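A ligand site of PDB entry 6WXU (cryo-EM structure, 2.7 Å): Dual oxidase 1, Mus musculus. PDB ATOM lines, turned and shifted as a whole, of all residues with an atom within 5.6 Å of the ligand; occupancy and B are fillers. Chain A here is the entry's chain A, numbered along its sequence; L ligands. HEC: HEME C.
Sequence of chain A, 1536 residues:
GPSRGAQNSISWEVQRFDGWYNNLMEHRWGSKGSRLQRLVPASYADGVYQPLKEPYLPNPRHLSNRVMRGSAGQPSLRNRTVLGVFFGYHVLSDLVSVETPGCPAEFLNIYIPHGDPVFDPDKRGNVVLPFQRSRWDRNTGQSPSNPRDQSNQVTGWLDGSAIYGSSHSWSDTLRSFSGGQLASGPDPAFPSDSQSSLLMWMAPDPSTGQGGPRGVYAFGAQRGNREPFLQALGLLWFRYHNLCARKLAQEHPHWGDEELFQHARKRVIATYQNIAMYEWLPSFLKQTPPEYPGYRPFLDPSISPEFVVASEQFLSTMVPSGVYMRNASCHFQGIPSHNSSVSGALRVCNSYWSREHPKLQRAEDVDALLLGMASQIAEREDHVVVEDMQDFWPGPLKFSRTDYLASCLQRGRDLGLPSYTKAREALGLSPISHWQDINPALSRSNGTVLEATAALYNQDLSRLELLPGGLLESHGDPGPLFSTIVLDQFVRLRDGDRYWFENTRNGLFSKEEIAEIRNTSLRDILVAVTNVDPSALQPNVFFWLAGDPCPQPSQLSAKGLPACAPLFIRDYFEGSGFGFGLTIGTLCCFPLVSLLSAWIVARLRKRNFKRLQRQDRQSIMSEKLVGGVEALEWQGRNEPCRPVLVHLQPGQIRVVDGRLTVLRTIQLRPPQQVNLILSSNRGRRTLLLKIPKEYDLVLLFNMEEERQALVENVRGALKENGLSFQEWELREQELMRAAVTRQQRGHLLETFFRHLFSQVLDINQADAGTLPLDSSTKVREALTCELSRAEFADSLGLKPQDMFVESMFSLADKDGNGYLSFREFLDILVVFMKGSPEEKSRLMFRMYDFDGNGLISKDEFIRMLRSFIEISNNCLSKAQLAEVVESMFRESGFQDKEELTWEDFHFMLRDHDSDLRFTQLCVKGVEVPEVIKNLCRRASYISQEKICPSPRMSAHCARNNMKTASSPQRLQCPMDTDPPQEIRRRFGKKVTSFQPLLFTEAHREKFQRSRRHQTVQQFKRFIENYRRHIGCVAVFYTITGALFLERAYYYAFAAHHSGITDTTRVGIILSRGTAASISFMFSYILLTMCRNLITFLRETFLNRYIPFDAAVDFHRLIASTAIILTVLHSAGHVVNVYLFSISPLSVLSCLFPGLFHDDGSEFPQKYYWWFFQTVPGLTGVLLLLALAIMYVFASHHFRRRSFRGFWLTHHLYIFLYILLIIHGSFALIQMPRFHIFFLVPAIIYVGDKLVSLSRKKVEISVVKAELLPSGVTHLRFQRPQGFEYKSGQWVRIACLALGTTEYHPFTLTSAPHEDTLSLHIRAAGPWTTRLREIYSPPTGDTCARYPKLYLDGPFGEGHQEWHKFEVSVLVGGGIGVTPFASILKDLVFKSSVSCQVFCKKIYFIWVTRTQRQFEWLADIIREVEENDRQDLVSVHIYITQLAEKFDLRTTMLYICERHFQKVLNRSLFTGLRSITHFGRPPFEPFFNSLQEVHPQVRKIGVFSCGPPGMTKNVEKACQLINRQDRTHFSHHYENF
An iron atom (FE) of the ligand is bound by a ring nitrogen (NE2) of His 1115 (2.2 Å).
FE of the ligand is bound by NE2 of His 1210.
An oxygen (O2A) of the ligand lies within salt-bridge range of the guanidinium group (NH2) of Arg 1091 (2.5 Å).
An oxygen (O2D) of the ligand lies within salt-bridge range of the side-chain amino group of Lys 1249 (2.8 Å).
OH of Tyr 1245 is in hydrogen-bond range of O2D of the ligand, 3.1 Å away.
Residues that only touch the ligand: Trp 1207, Ala 1194, Arg 1116, Ala 1119, Tyr 1191, Met 1190, Ile 1085, Tyr 1217, Met 1089, Phe 1206, Tyr 1213, Arg 1199 and Leu 1086.
18 residues have an atom within 4 Å of the ligand: Ile 1085, Leu 1086, Met 1089, Arg 1091, His 1115, Arg 1116, Ala 1119, Met 1190, Tyr 1191, Ala 1194, Arg 1199, Phe 1206, Trp 1207, His 1210, Tyr 1213, Tyr 1217, Tyr 1245 and Lys 1249.
The nearest printed residue that does not touch the ligand is Phe 1082 (4.1 Å).
OH of Tyr 1245 sits at hydrogen-bond distance from OH of Tyr 1213, 3.2 Å away.
The backbone carbonyl oxygen (O) of Arg 1116 sits at hydrogen-bond distance from the side-chain hydroxyl (OG) of Ser 1120 (3.0 Å).
The side-chain hydroxyl (OH) of Tyr 1191 sits at hydrogen-bond distance from the backbone carbonyl oxygen (O) of Ala 1119, at 2.4 Å.
The side-chain hydroxyl (OH) of Tyr 1217 sits at hydrogen-bond distance from the backbone carbonyl oxygen (O) of Phe 1082, at 2.4 Å.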
ATOM      1  N   PHE A1082      -9.450  -3.762  31.011  1.00  0.00           N
ATOM      2  CA  PHE A1082     -10.141  -3.307  29.814  1.00  0.00           C
ATOM      3  C   PHE A1082      -9.216  -3.124  28.626  1.00  0.00           C
ATOM      4  O   PHE A1082      -9.679  -3.144  27.478  1.00  0.00           O
ATOM      5  CB  PHE A1082     -10.876  -1.992  30.082  1.00  0.00           C
ATOM      6  CG  PHE A1082     -12.194  -2.175  30.787  1.00  0.00           C
ATOM      7  CD1 PHE A1082     -13.112  -3.102  30.338  1.00  0.00           C
ATOM      8  CD2 PHE A1082     -12.509  -1.418  31.896  1.00  0.00           C
ATOM      9  CE1 PHE A1082     -14.316  -3.268  30.984  1.00  0.00           C
ATOM     10  CE2 PHE A1082     -13.703  -1.586  32.540  1.00  0.00           C
ATOM     11  CZ  PHE A1082     -14.611  -2.513  32.089  1.00  0.00           C
ATOM     12  N   ILE A1085      -8.135  -6.917  27.203  1.00  0.00           N
ATOM     13  CA  ILE A1085      -9.209  -7.844  26.855  1.00  0.00           C
ATOM     14  C   ILE A1085      -9.336  -8.034  25.351  1.00  0.00           C
ATOM     15  O   ILE A1085     -10.129  -8.865  24.904  1.00  0.00           O
ATOM     16  CB  ILE A1085     -10.545  -7.344  27.456  1.00  0.00           C
ATOM     17  CG1 ILE A1085     -11.480  -8.517  27.709  1.00  0.00           C
ATOM     18  CG2 ILE A1085     -11.206  -6.358  26.528  1.00  0.00           C
ATOM     19  CD1 ILE A1085     -12.785  -8.112  28.320  1.00  0.00           C
ATOM     20  N   LEU A1086      -8.570  -7.292  24.561  1.00  0.00           N
ATOM     21  CA  LEU A1086      -8.562  -7.454  23.107  1.00  0.00           C
ATOM     22  C   LEU A1086      -7.576  -8.505  22.633  1.00  0.00           C
ATOM     23  O   LEU A1086      -7.724  -9.017  21.514  1.00  0.00           O
ATOM     24  CB  LEU A1086      -8.245  -6.116  22.433  1.00  0.00           C
ATOM     25  CG  LEU A1086      -9.111  -4.926  22.855  1.00  0.00           C
ATOM     26  CD1 LEU A1086      -8.569  -3.647  22.282  1.00  0.00           C
ATOM     27  CD2 LEU A1086     -10.536  -5.136  22.404  1.00  0.00           C
ATOM     28  N   MET A1089      -9.255 -11.591  21.604  1.00  0.00           N
ATOM     29  CA  MET A1089      -9.981 -11.579  20.337  1.00  0.00           C
ATOM     30  C   MET A1089      -9.080 -11.264  19.154  1.00  0.00           C
ATOM     31  O   MET A1089      -9.576 -11.091  18.036  1.00  0.00           O
ATOM     32  CB  MET A1089     -11.151 -10.598  20.398  1.00  0.00           C
ATOM     33  CG  MET A1089     -12.374 -11.158  21.089  1.00  0.00           C
ATOM     34  SD  MET A1089     -12.635 -12.888  20.673  1.00  0.00           S
ATOM     35  CE  MET A1089     -14.112 -13.265  21.596  1.00  0.00           C
ATOM     36  N   ARG A1091      -7.729 -12.748  16.658  1.00  0.00           N
ATOM     37  CA  ARG A1091      -7.966 -14.108  16.190  1.00  0.00           C
ATOM     38  C   ARG A1091      -6.832 -14.641  15.335  1.00  0.00           C
ATOM     39  O   ARG A1091      -6.423 -15.794  15.482  1.00  0.00           O
ATOM     40  CB  ARG A1091      -9.287 -14.175  15.422  1.00  0.00           C
ATOM     41  CG  ARG A1091     -10.465 -13.601  16.172  1.00  0.00           C
ATOM     42  CD  ARG A1091     -11.712 -13.581  15.301  1.00  0.00           C
ATOM     43  NE  ARG A1091     -12.812 -12.851  15.925  1.00  0.00           N
ATOM     44  CZ  ARG A1091     -13.733 -13.415  16.704  1.00  0.00           C
ATOM     45  NH1 ARG A1091     -13.680 -14.719  16.964  1.00  0.00           N
ATOM     46  NH2 ARG A1091     -14.700 -12.683  17.216  1.00  0.00           N
ATOM     47  N   VAL A1112     -12.122 -17.660  24.356  1.00  0.00           N
ATOM     48  CA  VAL A1112     -13.380 -16.959  24.572  1.00  0.00           C
ATOM     49  C   VAL A1112     -13.874 -17.146  26.004  1.00  0.00           C
ATOM     50  O   VAL A1112     -14.482 -16.242  26.574  1.00  0.00           O
ATOM     51  CB  VAL A1112     -14.434 -17.426  23.564  1.00  0.00           C
ATOM     52  CG1 VAL A1112     -15.750 -16.704  23.789  1.00  0.00           C
ATOM     53  CG2 VAL A1112     -13.943 -17.200  22.151  1.00  0.00           C
ATOM     54  N   HIS A1115     -12.398 -14.575  27.728  1.00  0.00           N
ATOM     55  CA  HIS A1115     -12.989 -13.305  27.459  1.00  0.00           C
ATOM     56  C   HIS A1115     -14.091 -13.078  28.413  1.00  0.00           C
ATOM     57  O   HIS A1115     -14.288 -11.992  28.812  1.00  0.00           O
ATOM     58  CB  HIS A1115     -13.485 -13.258  26.021  1.00  0.00           C
ATOM     59  CG  HIS A1115     -14.054 -11.976  25.581  1.00  0.00           C
ATOM     60  ND1 HIS A1115     -13.285 -10.941  25.128  1.00  0.00           N
ATOM     61  CD2 HIS A1115     -15.319 -11.602  25.406  1.00  0.00           C
ATOM     62  CE1 HIS A1115     -14.069  -9.951  24.766  1.00  0.00           C
ATOM     63  NE2 HIS A1115     -15.322 -10.343  24.888  1.00  0.00           N
ATOM     64  N   ARG A1116     -14.863 -14.081  28.776  1.00  0.00           N
ATOM     65  CA  ARG A1116     -15.981 -13.830  29.621  1.00  0.00           C
ATOM     66  C   ARG A1116     -15.633 -13.788  31.027  1.00  0.00           C
ATOM     67  O   ARG A1116     -16.441 -13.437  31.824  1.00  0.00           O
ATOM     68  CB  ARG A1116     -16.987 -14.878  29.390  1.00  0.00           C
ATOM     69  CG  ARG A1116     -17.157 -15.092  27.947  1.00  0.00           C
ATOM     70  CD  ARG A1116     -18.516 -15.622  27.684  1.00  0.00           C
ATOM     71  NE  ARG A1116     -18.501 -17.041  27.804  1.00  0.00           N
ATOM     72  CZ  ARG A1116     -18.544 -17.658  28.956  1.00  0.00           C
ATOM     73  NH1 ARG A1116     -18.620 -16.940  30.052  1.00  0.00           N
ATOM     74  NH2 ARG A1116     -18.516 -18.970  29.019  1.00  0.00           N
ATOM     75  N   ALA A1119     -14.098 -10.207  31.488  1.00  0.00           N
ATOM     76  CA  ALA A1119     -15.164  -9.227  31.333  1.00  0.00           C
ATOM     77  C   ALA A1119     -16.092  -9.200  32.536  1.00  0.00           C
ATOM     78  O   ALA A1119     -16.545  -8.131  32.943  1.00  0.00           O
ATOM     79  CB  ALA A1119     -15.945  -9.510  30.065  1.00  0.00           C
ATOM     80  N   SER A1120     -16.385 -10.360  33.107  1.00  0.00           N
ATOM     81  CA  SER A1120     -17.285 -10.437  34.249  1.00  0.00           C
ATOM     82  C   SER A1120     -16.563 -10.220  35.572  1.00  0.00           C
ATOM     83  O   SER A1120     -17.215 -10.218  36.616  1.00  0.00           O
ATOM     84  CB  SER A1120     -17.993 -11.781  34.282  1.00  0.00           C
ATOM     85  OG  SER A1120     -17.106 -12.807  34.671  1.00  0.00           O
ATOM     86  N   LEU A1187     -21.998   0.237  29.595  1.00  0.00           N
ATOM     87  CA  LEU A1187     -21.739  -1.085  30.157  1.00  0.00           C
ATOM     88  C   LEU A1187     -23.028  -1.801  30.523  1.00  0.00           C
ATOM     89  O   LEU A1187     -23.135  -3.016  30.341  1.00  0.00           O
ATOM     90  CB  LEU A1187     -20.832  -0.970  31.383  1.00  0.00           C
ATOM     91  CG  LEU A1187     -19.402  -0.513  31.119  1.00  0.00           C
ATOM     92  CD1 LEU A1187     -18.656  -0.421  32.429  1.00  0.00           C
ATOM     93  CD2 LEU A1187     -18.709  -1.482  30.207  1.00  0.00           C
ATOM     94  N   MET A1190     -24.239  -3.149  27.164  1.00  0.00           N
ATOM     95  CA  MET A1190     -23.337  -4.095  26.549  1.00  0.00           C
ATOM     96  C   MET A1190     -23.267  -5.409  27.313  1.00  0.00           C
ATOM     97  O   MET A1190     -23.038  -6.458  26.723  1.00  0.00           O
ATOM     98  CB  MET A1190     -21.954  -3.465  26.428  1.00  0.00           C
ATOM     99  CG  MET A1190     -20.946  -4.267  25.676  1.00  0.00           C
ATOM    100  SD  MET A1190     -19.392  -3.390  25.597  1.00  0.00           S
ATOM    101  CE  MET A1190     -18.505  -4.410  24.436  1.00  0.00           C
ATOM    102  N   TYR A1191     -23.466  -5.367  28.635  1.00  0.00           N
ATOM    103  CA  TYR A1191     -23.390  -6.586  29.424  1.00  0.00           C
ATOM    104  C   TYR A1191     -24.700  -7.347  29.473  1.00  0.00           C
ATOM    105  O   TYR A1191     -24.699  -8.575  29.503  1.00  0.00           O
ATOM    106  CB  TYR A1191     -22.953  -6.263  30.855  1.00  0.00           C
ATOM    107  CG  TYR A1191     -21.464  -6.262  31.056  1.00  0.00           C
ATOM    108  CD1 TYR A1191     -20.665  -5.303  30.475  1.00  0.00           C
ATOM    109  CD2 TYR A1191     -20.862  -7.241  31.827  1.00  0.00           C
ATOM    110  CE1 TYR A1191     -19.314  -5.299  30.650  1.00  0.00           C
ATOM    111  CE2 TYR A1191     -19.500  -7.244  32.008  1.00  0.00           C
ATOM    112  CZ  TYR A1191     -18.731  -6.275  31.425  1.00  0.00           C
ATOM    113  OH  TYR A1191     -17.379  -6.271  31.600  1.00  0.00           O
ATOM    114  N   ALA A1194     -25.197  -8.926  25.857  1.00  0.00           N
ATOM    115  CA  ALA A1194     -24.228  -9.993  25.641  1.00  0.00           C
ATOM    116  C   ALA A1194     -24.283 -11.014  26.767  1.00  0.00           C
ATOM    117  O   ALA A1194     -23.270 -11.375  27.357  1.00  0.00           O
ATOM    118  CB  ALA A1194     -22.823  -9.424  25.507  1.00  0.00           C
ATOM    119  N   SER A1195     -25.484 -11.495  27.069  1.00  0.00           N
ATOM    120  CA  SER A1195     -25.709 -12.466  28.121  1.00  0.00           C
ATOM    121  C   SER A1195     -26.181 -13.785  27.512  1.00  0.00           C
ATOM    122  O   SER A1195     -26.876 -13.808  26.497  1.00  0.00           O
ATOM    123  CB  SER A1195     -26.750 -11.966  29.121  1.00  0.00           C
ATOM    124  OG  SER A1195     -27.048 -12.970  30.074  1.00  0.00           O
ATOM    125  N   ARG A1199     -28.087 -13.729  24.244  1.00  0.00           N
ATOM    126  CA  ARG A1199     -27.244 -14.061  23.112  1.00  0.00           C
ATOM    127  C   ARG A1199     -27.703 -15.346  22.440  1.00  0.00           C
ATOM    128  O   ARG A1199     -27.560 -15.512  21.229  1.00  0.00           O
ATOM    129  CB  ARG A1199     -25.794 -14.160  23.570  1.00  0.00           C
ATOM    130  CG  ARG A1199     -24.849 -14.805  22.589  1.00  0.00           C
ATOM    131  CD  ARG A1199     -23.407 -14.518  22.971  1.00  0.00           C
ATOM    132  NE  ARG A1199     -23.138 -14.791  24.374  1.00  0.00           N
ATOM    133  CZ  ARG A1199     -22.633 -15.936  24.827  1.00  0.00           C
ATOM    134  NH1 ARG A1199     -22.338 -16.902  23.976  1.00  0.00           N
ATOM    135  NH2 ARG A1199     -22.422 -16.109  26.123  1.00  0.00           N
ATOM    136  N   PHE A1206     -27.434  -8.858  20.147  1.00  0.00           N
ATOM    137  CA  PHE A1206     -26.122  -8.981  20.763  1.00  0.00           C
ATOM    138  C   PHE A1206     -25.043  -8.382  19.870  1.00  0.00           C
ATOM    139  O   PHE A1206     -24.175  -7.642  20.342  1.00  0.00           O
ATOM    140  CB  PHE A1206     -25.806 -10.443  21.054  1.00  0.00           C
ATOM    141  CG  PHE A1206     -24.340 -10.758  21.054  1.00  0.00           C
ATOM    142  CD1 PHE A1206     -23.544 -10.401  22.123  1.00  0.00           C
ATOM    143  CD2 PHE A1206     -23.769 -11.412  19.994  1.00  0.00           C
ATOM    144  CE1 PHE A1206     -22.197 -10.690  22.128  1.00  0.00           C
ATOM    145  CE2 PHE A1206     -22.425 -11.703  19.985  1.00  0.00           C
ATOM    146  CZ  PHE A1206     -21.638 -11.344  21.056  1.00  0.00           C
ATOM    147  N   TRP A1207     -25.085  -8.677  18.571  1.00  0.00           N
ATOM    148  CA  TRP A1207     -24.025  -8.227  17.676  1.00  0.00           C
ATOM    149  C   TRP A1207     -24.034  -6.720  17.524  1.00  0.00           C
ATOM    150  O   TRP A1207     -22.969  -6.096  17.398  1.00  0.00           O
ATOM    151  CB  TRP A1207     -24.164  -8.906  16.320  1.00  0.00           C
ATOM    152  CG  TRP A1207     -22.950  -8.780  15.474  1.00  0.00           C
ATOM    153  CD1 TRP A1207     -22.853  -8.147  14.266  1.00  0.00           C
ATOM    154  CD2 TRP A1207     -21.647  -9.272  15.769  1.00  0.00           C
ATOM    155  NE1 TRP A1207     -21.566  -8.231  13.797  1.00  0.00           N
ATOM    156  CE2 TRP A1207     -20.814  -8.922  14.697  1.00  0.00           C
ATOM    157  CE3 TRP A1207     -21.114  -9.999  16.838  1.00  0.00           C
ATOM    158  CZ2 TRP A1207     -19.459  -9.259  14.662  1.00  0.00           C
ATOM    159  CZ3 TRP A1207     -19.779 -10.334  16.807  1.00  0.00           C
ATOM    160  CH2 TRP A1207     -18.965  -9.961  15.728  1.00  0.00           C
ATOM    161  N   HIS A1210     -22.935  -5.104  20.992  1.00  0.00           N
ATOM    162  CA  HIS A1210     -21.564  -5.405  21.370  1.00  0.00           C
ATOM    163  C   HIS A1210     -20.555  -4.534  20.650  1.00  0.00           C
ATOM    164  O   HIS A1210     -19.364  -4.619  20.960  1.00  0.00           O
ATOM    165  CB  HIS A1210     -21.249  -6.874  21.091  1.00  0.00           C
ATOM    166  CG  HIS A1210     -20.268  -7.465  22.052  1.00  0.00           C
ATOM    167  ND1 HIS A1210     -20.630  -7.956  23.281  1.00  0.00           N
ATOM    168  CD2 HIS A1210     -18.923  -7.629  21.964  1.00  0.00           C
ATOM    169  CE1 HIS A1210     -19.558  -8.404  23.913  1.00  0.00           C
ATOM    170  NE2 HIS A1210     -18.510  -8.218  23.128  1.00  0.00           N
ATOM    171  N   TYR A1213     -18.004  -1.122  22.216  1.00  0.00           N
ATOM    172  CA  TYR A1213     -16.665  -1.031  22.783  1.00  0.00           C
ATOM    173  C   TYR A1213     -15.865   0.099  22.147  1.00  0.00           C
ATOM    174  O   TYR A1213     -14.959   0.643  22.792  1.00  0.00           O
ATOM    175  CB  TYR A1213     -15.925  -2.364  22.668  1.00  0.00           C
ATOM    176  CG  TYR A1213     -15.605  -2.795  21.255  1.00  0.00           C
ATOM    177  CD1 TYR A1213     -16.511  -3.536  20.516  1.00  0.00           C
ATOM    178  CD2 TYR A1213     -14.393  -2.479  20.665  1.00  0.00           C
ATOM    179  CE1 TYR A1213     -16.226  -3.940  19.231  1.00  0.00           C
ATOM    180  CE2 TYR A1213     -14.097  -2.876  19.384  1.00  0.00           C
ATOM    181  CZ  TYR A1213     -15.018  -3.606  18.668  1.00  0.00           C
ATOM    182  OH  TYR A1213     -14.719  -3.996  17.393  1.00  0.00           O
ATOM    183  N   LEU A1216     -16.872   2.896  24.024  1.00  0.00           N
ATOM    184  CA  LEU A1216     -16.359   2.693  25.374  1.00  0.00           C
ATOM    185  C   LEU A1216     -14.920   3.176  25.489  1.00  0.00           C
ATOM    186  O   LEU A1216     -14.564   3.863  26.448  1.00  0.00           O
ATOM    187  CB  LEU A1216     -16.451   1.216  25.738  1.00  0.00           C
ATOM    188  CG  LEU A1216     -16.583   0.892  27.223  1.00  0.00           C
ATOM    189  CD1 LEU A1216     -18.016   1.048  27.632  1.00  0.00           C
ATOM    190  CD2 LEU A1216     -16.092  -0.512  27.482  1.00  0.00           C
ATOM    191  N   TYR A1217     -14.071   2.808  24.533  1.00  0.00           N
ATOM    192  CA  TYR A1217     -12.677   3.232  24.606  1.00  0.00           C
ATOM    193  C   TYR A1217     -12.530   4.714  24.318  1.00  0.00           C
ATOM    194  O   TYR A1217     -11.627   5.368  24.872  1.00  0.00           O
ATOM    195  CB  TYR A1217     -11.823   2.399  23.648  1.00  0.00           C
ATOM    196  CG  TYR A1217     -11.609   0.992  24.134  1.00  0.00           C
ATOM    197  CD1 TYR A1217     -10.837   0.735  25.252  1.00  0.00           C
ATOM    198  CD2 TYR A1217     -12.173  -0.081  23.473  1.00  0.00           C
ATOM    199  CE1 TYR A1217     -10.645  -0.545  25.699  1.00  0.00           C
ATOM    200  CE2 TYR A1217     -11.993  -1.361  23.908  1.00  0.00           C
ATOM    201  CZ  TYR A1217     -11.228  -1.590  25.024  1.00  0.00           C
ATOM    202  OH  TYR A1217     -11.038  -2.877  25.466  1.00  0.00           O
ATOM    203  N   TYR A1245      -4.530  -5.349  18.029  1.00  0.00           N
ATOM    204  CA  TYR A1245      -5.889  -5.675  17.622  1.00  0.00           C
ATOM    205  C   TYR A1245      -6.209  -5.101  16.246  1.00  0.00           C
ATOM    206  O   TYR A1245      -6.761  -5.791  15.390  1.00  0.00           O
ATOM    207  CB  TYR A1245      -6.881  -5.169  18.662  1.00  0.00           C
ATOM    208  CG  TYR A1245      -8.325  -5.423  18.306  1.00  0.00           C
ATOM    209  CD1 TYR A1245      -8.886  -6.672  18.467  1.00  0.00           C
ATOM    210  CD2 TYR A1245      -9.126  -4.402  17.829  1.00  0.00           C
ATOM    211  CE1 TYR A1245     -10.199  -6.913  18.150  1.00  0.00           C
ATOM    212  CE2 TYR A1245     -10.437  -4.629  17.510  1.00  0.00           C
ATOM    213  CZ  TYR A1245     -10.969  -5.882  17.666  1.00  0.00           C
ATOM    214  OH  TYR A1245     -12.280  -6.115  17.355  1.00  0.00           O
ATOM    215  N   LYS A1249      -6.946  -6.939  12.776  1.00  0.00           N
ATOM    216  CA  LYS A1249      -8.190  -6.646  12.085  1.00  0.00           C
ATOM    217  C   LYS A1249      -7.940  -6.304  10.618  1.00  0.00           C
ATOM    218  O   LYS A1249      -8.708  -6.711   9.737  1.00  0.00           O
ATOM    219  CB  LYS A1249      -8.922  -5.507  12.776  1.00  0.00           C
ATOM    220  CG  LYS A1249     -10.432  -5.580  12.674  1.00  0.00           C
ATOM    221  CD  LYS A1249     -10.954  -6.800  13.382  1.00  0.00           C
ATOM    222  CE  LYS A1249     -12.467  -6.842  13.357  1.00  0.00           C
ATOM    223  NZ  LYS A1249     -12.992  -8.051  14.036  1.00  0.00           N
HETATM  224 FE   HEC L   1     -17.333  -9.724  24.316  1.00  0.00          FE
HETATM  225  CHA HEC L   1     -16.566 -10.647  20.982  1.00  0.00           C
HETATM  226  CHB HEC L   1     -19.081 -12.372  24.789  1.00  0.00           C
HETATM  227  CHC HEC L   1     -17.828  -8.457  27.403  1.00  0.00           C
HETATM  228  CHD HEC L   1     -15.244  -6.793  23.619  1.00  0.00           C
HETATM  229  NA  HEC L   1     -17.688 -11.163  23.126  1.00  0.00           N
HETATM  230  C1A HEC L   1     -17.362 -11.399  21.844  1.00  0.00           C
HETATM  231  C2A HEC L   1     -17.967 -12.561  21.411  1.00  0.00           C
HETATM  232  C3A HEC L   1     -18.692 -13.049  22.492  1.00  0.00           C
HETATM  233  C4A HEC L   1     -18.472 -12.179  23.544  1.00  0.00           C
HETATM  234  CMA HEC L   1     -19.546 -14.289  22.556  1.00  0.00           C
HETATM  235  CAA HEC L   1     -17.864 -13.112  20.009  1.00  0.00           C
HETATM  236  CBA HEC L   1     -17.252 -14.502  19.961  1.00  0.00           C
HETATM  237  CGA HEC L   1     -17.266 -14.954  18.521  1.00  0.00           C
HETATM  238  O1A HEC L   1     -18.104 -15.875  18.172  1.00  0.00           O
HETATM  239  O2A HEC L   1     -16.483 -14.413  17.735  1.00  0.00           O
HETATM  240  NB  HEC L   1     -18.226 -10.265  25.754  1.00  0.00           N
HETATM  241  C1B HEC L   1     -18.911 -11.425  25.791  1.00  0.00           C
HETATM  242  C2B HEC L   1     -19.508 -11.597  27.038  1.00  0.00           C
HETATM  243  C3B HEC L   1     -19.132 -10.463  27.750  1.00  0.00           C
HETATM  244  C4B HEC L   1     -18.350  -9.666  26.951  1.00  0.00           C
HETATM  245  CMB HEC L   1     -20.348 -12.764  27.468  1.00  0.00           C
HETATM  246  CAB HEC L   1     -19.464 -10.112  29.152  1.00  0.00           C
HETATM  247  CBB HEC L   1     -20.601 -10.452  29.717  1.00  0.00           C
HETATM  248  NC  HEC L   1     -16.658  -7.994  25.277  1.00  0.00           N
HETATM  249  C1C HEC L   1     -17.030  -7.698  26.547  1.00  0.00           C
HETATM  250  C2C HEC L   1     -16.488  -6.485  26.936  1.00  0.00           C
HETATM  251  C3C HEC L   1     -15.763  -6.057  25.833  1.00  0.00           C
HETATM  252  C4C HEC L   1     -15.889  -6.979  24.833  1.00  0.00           C
HETATM  253  CMC HEC L   1     -16.658  -5.799  28.271  1.00  0.00           C
HETATM  254  CAC HEC L   1     -14.986  -4.806  25.681  1.00  0.00           C
HETATM  255  CBC HEC L   1     -14.122  -4.418  26.589  1.00  0.00           C
HETATM  256  ND  HEC L   1     -16.140  -8.877  22.637  1.00  0.00           N
HETATM  257  C1D HEC L   1     -15.413  -7.747  22.624  1.00  0.00           C
HETATM  258  C2D HEC L   1     -14.795  -7.602  21.404  1.00  0.00           C
HETATM  259  C3D HEC L   1     -15.164  -8.686  20.642  1.00  0.00           C
HETATM  260  C4D HEC L   1     -15.995  -9.470  21.442  1.00  0.00           C
HETATM  261  CMD HEC L   1     -13.890  -6.485  20.967  1.00  0.00           C
HETATM  262  CAD HEC L   1     -14.713  -8.971  19.233  1.00  0.00           C
HETATM  263  CBD HEC L   1     -15.831  -8.655  18.255  1.00  0.00           C
HETATM  264  CGD HEC L   1     -15.318  -8.880  16.863  1.00  0.00           C
HETATM  265  O1D HEC L   1     -15.873  -9.802  16.156  1.00  0.00           O
HETATM  266  O2D HEC L   1     -14.384  -8.176  16.465  1.00  0.00           O
